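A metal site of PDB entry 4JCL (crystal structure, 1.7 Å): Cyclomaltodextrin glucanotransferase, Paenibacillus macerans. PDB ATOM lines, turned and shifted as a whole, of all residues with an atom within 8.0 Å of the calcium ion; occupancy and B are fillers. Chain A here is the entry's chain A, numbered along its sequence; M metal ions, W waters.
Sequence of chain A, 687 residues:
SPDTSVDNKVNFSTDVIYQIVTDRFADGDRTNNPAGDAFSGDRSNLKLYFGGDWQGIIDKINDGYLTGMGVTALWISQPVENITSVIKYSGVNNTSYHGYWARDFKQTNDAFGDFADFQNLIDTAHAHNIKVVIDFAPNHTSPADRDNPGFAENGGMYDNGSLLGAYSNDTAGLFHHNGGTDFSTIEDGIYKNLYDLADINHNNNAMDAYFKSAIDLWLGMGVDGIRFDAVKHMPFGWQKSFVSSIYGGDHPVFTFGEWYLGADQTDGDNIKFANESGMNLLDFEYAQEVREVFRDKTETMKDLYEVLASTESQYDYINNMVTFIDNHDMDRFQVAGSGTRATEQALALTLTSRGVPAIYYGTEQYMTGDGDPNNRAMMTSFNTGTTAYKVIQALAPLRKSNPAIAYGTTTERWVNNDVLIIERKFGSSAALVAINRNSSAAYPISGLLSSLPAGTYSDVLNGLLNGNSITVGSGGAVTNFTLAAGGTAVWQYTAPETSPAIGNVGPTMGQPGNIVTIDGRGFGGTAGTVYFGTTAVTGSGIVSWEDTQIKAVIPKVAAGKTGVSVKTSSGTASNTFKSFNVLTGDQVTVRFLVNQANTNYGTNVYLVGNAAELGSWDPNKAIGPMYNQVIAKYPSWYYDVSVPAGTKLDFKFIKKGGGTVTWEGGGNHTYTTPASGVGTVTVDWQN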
ATOM      1  N   GLY A 262       3.788  -3.979 -16.530  1.00  0.00           N
ATOM      2  CA  GLY A 262       4.531  -3.692 -17.735  1.00  0.00           C
ATOM      3  C   GLY A 262       5.925  -3.170 -17.393  1.00  0.00           C
ATOM      4  O   GLY A 262       6.256  -3.017 -16.232  1.00  0.00           O
ATOM      5  N   ALA A 263       6.747  -2.930 -18.412  1.00  0.00           N
ATOM      6  CA  ALA A 263       8.018  -2.251 -18.196  1.00  0.00           C
ATOM      7  C   ALA A 263       7.794  -0.904 -17.498  1.00  0.00           C
ATOM      8  O   ALA A 263       6.780  -0.256 -17.700  1.00  0.00           O
ATOM      9  CB  ALA A 263       8.718  -2.025 -19.540  1.00  0.00           C
ATOM     10  N   ASP A 264       8.745  -0.496 -16.661  1.00  0.00           N
ATOM     11  CA  ASP A 264       8.714   0.854 -16.068  1.00  0.00           C
ATOM     12  C   ASP A 264       7.465   1.101 -15.236  1.00  0.00           C
ATOM     13  O   ASP A 264       6.941   2.221 -15.197  1.00  0.00           O
ATOM     14  CB  ASP A 264       8.779   1.917 -17.169  1.00  0.00           C
ATOM     15  CG  ASP A 264      10.027   1.816 -18.007  1.00  0.00           C
ATOM     16  OD1 ASP A 264       9.938   1.905 -19.243  1.00  0.00           O
ATOM     17  OD2 ASP A 264      11.106   1.632 -17.424  1.00  0.00           O
ATOM     18  N   GLN A 265       6.982   0.078 -14.564  1.00  0.00           N
ATOM     19  CA  GLN A 265       5.769   0.245 -13.790  1.00  0.00           C
ATOM     20  C   GLN A 265       5.939  -0.309 -12.398  1.00  0.00           C
ATOM     21  O   GLN A 265       6.423  -1.436 -12.199  1.00  0.00           O
ATOM     22  CB  GLN A 265       4.567  -0.425 -14.474  1.00  0.00           C
ATOM     23  CG  GLN A 265       3.249  -0.236 -13.738  1.00  0.00           C
ATOM     24  CD  GLN A 265       2.096  -1.055 -14.318  1.00  0.00           C
ATOM     25  OE1 GLN A 265       2.257  -1.763 -15.307  1.00  0.00           O
ATOM     26  NE2 GLN A 265       0.935  -0.956 -13.685  1.00  0.00           N
ATOM     27  N   GLU A 285       8.515  -6.533 -11.800  1.00  0.00           N
ATOM     28  CA  GLU A 285       9.466  -5.418 -11.803  1.00  0.00           C
ATOM     29  C   GLU A 285      10.872  -5.893 -12.150  1.00  0.00           C
ATOM     30  O   GLU A 285      11.565  -5.269 -12.966  1.00  0.00           O
ATOM     31  CB  GLU A 285       9.462  -4.660 -10.480  1.00  0.00           C
ATOM     32  CG  GLU A 285       8.250  -3.758 -10.318  1.00  0.00           C
ATOM     33  CD  GLU A 285       8.451  -2.727  -9.235  1.00  0.00           C
ATOM     34  OE1 GLU A 285       7.563  -2.621  -8.354  1.00  0.00           O
ATOM     35  OE2 GLU A 285       9.474  -2.025  -9.262  1.00  0.00           O
ATOM     36  N   GLN A 288      10.762  -7.356 -16.015  1.00  0.00           N
ATOM     37  CA  GLN A 288      10.708  -6.332 -17.049  1.00  0.00           C
ATOM     38  C   GLN A 288      12.034  -5.596 -17.118  1.00  0.00           C
ATOM     39  O   GLN A 288      12.490  -5.216 -18.209  1.00  0.00           O
ATOM     40  CB  GLN A 288       9.550  -5.336 -16.826  1.00  0.00           C
ATOM     41  CG  GLN A 288       8.134  -5.938 -16.898  1.00  0.00           C
ATOM     42  CD  GLN A 288       7.665  -6.286 -18.324  1.00  0.00           C
ATOM     43  OE1 GLN A 288       6.485  -6.534 -18.549  1.00  0.00           O
ATOM     44  NE2 GLN A 288       8.591  -6.312 -19.270  1.00  0.00           N
ATOM     45  N   GLU A 289      12.663  -5.362 -15.967  1.00  0.00           N
ATOM     46  CA  GLU A 289      13.909  -4.600 -15.954  1.00  0.00           C
ATOM     47  C   GLU A 289      15.058  -5.387 -16.562  1.00  0.00           C
ATOM     48  O   GLU A 289      15.855  -4.841 -17.329  1.00  0.00           O
ATOM     49  CB  GLU A 289      14.262  -4.159 -14.529  1.00  0.00           C
ATOM     50  CG  GLU A 289      15.514  -3.263 -14.473  1.00  0.00           C
ATOM     51  CD  GLU A 289      15.307  -1.941 -15.186  1.00  0.00           C
ATOM     52  OE1 GLU A 289      16.300  -1.369 -15.698  1.00  0.00           O
ATOM     53  OE2 GLU A 289      14.153  -1.474 -15.248  1.00  0.00           O
ATOM     54  N   VAL A 290      15.151  -6.669 -16.202  1.00  0.00           N
ATOM     55  CA  VAL A 290      16.153  -7.537 -16.802  1.00  0.00           C
ATOM     56  C   VAL A 290      16.006  -7.538 -18.311  1.00  0.00           C
ATOM     57  O   VAL A 290      16.997  -7.495 -19.044  1.00  0.00           O
ATOM     58  CB  VAL A 290      16.058  -8.975 -16.240  1.00  0.00           C
ATOM     59  CG1 VAL A 290      16.882  -9.944 -17.062  1.00  0.00           C
ATOM     60  CG2 VAL A 290      16.523  -8.974 -14.784  1.00  0.00           C
ATOM     61  N   GLU A 292      14.729  -5.124 -20.228  1.00  0.00           N
ATOM     62  CA  GLU A 292      15.182  -3.849 -20.761  1.00  0.00           C
ATOM     63  C   GLU A 292      16.698  -3.802 -20.851  1.00  0.00           C
ATOM     64  O   GLU A 292      17.266  -3.308 -21.828  1.00  0.00           O
ATOM     65  CB  GLU A 292      14.700  -2.682 -19.908  1.00  0.00           C
ATOM     66  CG  GLU A 292      13.204  -2.501 -19.918  1.00  0.00           C
ATOM     67  CD  GLU A 292      12.815  -1.190 -19.339  1.00  0.00           C
ATOM     68  OE1 GLU A 292      12.458  -0.290 -20.114  1.00  0.00           O
ATOM     69  OE2 GLU A 292      12.879  -1.047 -18.103  1.00  0.00           O
ATOM     70  N   VAL A 293      17.353  -4.306 -19.814  1.00  0.00           N
ATOM     71  CA  VAL A 293      18.796  -4.161 -19.722  1.00  0.00           C
ATOM     72  C   VAL A 293      19.520  -5.149 -20.628  1.00  0.00           C
ATOM     73  O   VAL A 293      20.481  -4.767 -21.305  1.00  0.00           O
ATOM     74  CB  VAL A 293      19.272  -4.286 -18.259  1.00  0.00           C
ATOM     75  CG1 VAL A 293      20.800  -4.329 -18.172  1.00  0.00           C
ATOM     76  CG2 VAL A 293      18.687  -3.134 -17.446  1.00  0.00           C
ATOM     77  N   THR A 298      17.987  -1.107 -23.481  1.00  0.00           N
ATOM     78  CA  THR A 298      17.493   0.270 -23.433  1.00  0.00           C
ATOM     79  C   THR A 298      17.760   0.943 -22.100  1.00  0.00           C
ATOM     80  O   THR A 298      17.521   2.144 -21.944  1.00  0.00           O
ATOM     81  CB  THR A 298      15.983   0.323 -23.691  1.00  0.00           C
ATOM     82  OG1 THR A 298      15.330  -0.588 -22.793  1.00  0.00           O
ATOM     83  CG2 THR A 298      15.668  -0.055 -25.134  1.00  0.00           C
ATOM     84  N   GLU A 299      18.226   0.179 -21.128  1.00  0.00           N
ATOM     85  CA  GLU A 299      18.559   0.753 -19.825  1.00  0.00           C
ATOM     86  C   GLU A 299      19.866   0.147 -19.351  1.00  0.00           C
ATOM     87  O   GLU A 299      20.320  -0.850 -19.918  1.00  0.00           O
ATOM     88  CB  GLU A 299      17.450   0.508 -18.806  1.00  0.00           C
ATOM     89  CG  GLU A 299      16.207   1.335 -19.085  1.00  0.00           C
ATOM     90  CD  GLU A 299      15.228   1.339 -17.948  1.00  0.00           C
ATOM     91  OE1 GLU A 299      15.534   0.798 -16.876  1.00  0.00           O
ATOM     92  OE2 GLU A 299      14.133   1.871 -18.108  1.00  0.00           O
ATOM     93  N   THR A 300      20.454   0.738 -18.318  1.00  0.00           N
ATOM     94  CA  THR A 300      21.815   0.369 -17.909  1.00  0.00           C
ATOM     95  C   THR A 300      21.826  -0.503 -16.669  1.00  0.00           C
ATOM     96  O   THR A 300      20.804  -0.684 -16.012  1.00  0.00           O
ATOM     97  CB  THR A 300      22.646   1.619 -17.614  1.00  0.00           C
ATOM     98  OG1 THR A 300      22.220   2.186 -16.369  1.00  0.00           O
ATOM     99  CG2 THR A 300      22.475   2.659 -18.711  1.00  0.00           C
ATOM    100  N   ASP A 303      20.419   1.176 -13.725  1.00  0.00           N
ATOM    101  CA  ASP A 303      18.971   1.076 -13.651  1.00  0.00           C
ATOM    102  C   ASP A 303      18.561  -0.270 -13.053  1.00  0.00           C
ATOM    103  O   ASP A 303      17.628  -0.350 -12.255  1.00  0.00           O
ATOM    104  CB  ASP A 303      18.359   1.254 -15.038  1.00  0.00           C
ATOM    105  CG  ASP A 303      18.584   2.648 -15.592  1.00  0.00           C
ATOM    106  OD1 ASP A 303      18.268   3.617 -14.873  1.00  0.00           O
ATOM    107  OD2 ASP A 303      19.106   2.768 -16.716  1.00  0.00           O
ATOM    108  N   LEU A 304      19.272  -1.307 -13.458  1.00  0.00           N
ATOM    109  CA  LEU A 304      19.019  -2.646 -12.938  1.00  0.00           C
ATOM    110  C   LEU A 304      19.189  -2.679 -11.425  1.00  0.00           C
ATOM    111  O   LEU A 304      18.333  -3.213 -10.696  1.00  0.00           O
ATOM    112  CB  LEU A 304      19.961  -3.651 -13.604  1.00  0.00           C
ATOM    113  CG  LEU A 304      19.891  -5.107 -13.171  1.00  0.00           C
ATOM    114  CD1 LEU A 304      18.451  -5.626 -13.191  1.00  0.00           C
ATOM    115  CD2 LEU A 304      20.791  -5.939 -14.064  1.00  0.00           C
ATOM    116  N   GLU A 306      19.046  -0.165  -9.345  1.00  0.00           N
ATOM    117  CA  GLU A 306      17.999   0.674  -8.780  1.00  0.00           C
ATOM    118  C   GLU A 306      16.719  -0.115  -8.527  1.00  0.00           C
ATOM    119  O   GLU A 306      16.065   0.080  -7.496  1.00  0.00           O
ATOM    120  CB  GLU A 306      17.707   1.867  -9.705  1.00  0.00           C
ATOM    121  CG  GLU A 306      18.706   3.012  -9.561  1.00  0.00           C
ATOM    122  CD  GLU A 306      18.472   4.150 -10.549  1.00  0.00           C
ATOM    123  OE1 GLU A 306      17.413   4.162 -11.213  1.00  0.00           O
ATOM    124  OE2 GLU A 306      19.347   5.025 -10.661  1.00  0.00           O
ATOM    125  N   VAL A 307      16.354  -0.971  -9.470  1.00  0.00           N
ATOM    126  CA  VAL A 307      15.172  -1.812  -9.297  1.00  0.00           C
ATOM    127  C   VAL A 307      15.385  -2.870  -8.212  1.00  0.00           C
ATOM    128  O   VAL A 307      14.480  -3.147  -7.420  1.00  0.00           O
ATOM    129  CB  VAL A 307      14.713  -2.467 -10.617  1.00  0.00           C
ATOM    130  CG1 VAL A 307      13.583  -3.451 -10.361  1.00  0.00           C
ATOM    131  CG2 VAL A 307      14.249  -1.398 -11.602  1.00  0.00           C
HETATM  132 CA    CA M   1      13.020   0.594 -16.223  1.00  0.00          CA
HETATM  133  O   HOH W   1      14.123   2.188 -14.165  1.00  0.00           O
HETATM  134  O   HOH W   2      11.458   0.186 -14.296  1.00  0.00           O
HETATM  135  O   HOH W   3      11.165  -2.034 -16.540  1.00  0.00           O
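O of Glu 292 is in hydrogen-bond range of N of Thr 298, 2.8 Å away.
Within 4 Å of the calcium ion: Asp 264, Glu 289, Glu 292 and Glu 299. Along chain A the residues within 4 Å of the calcium ion span positions 264 to 299. The nearest printed residue that does not touch the calcium ion is Val 307 (5.2 Å).
The calcium ion is bound by the side-chain carboxylate (OD2) of Asp 264 (2.5 Å), the side-chain carboxylate (OE2) of Glu 292 (2.5 Å), water W2 (2.5 Å), the side-chain carboxylate (OE2) of Glu 299 (2.5 Å), the side-chain carboxylate (OE2) of Glu 289 (2.6 Å), the side-chain carboxylate (OE1) of Glu 299 (2.6 Å) and water W1 (2.8 Å).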
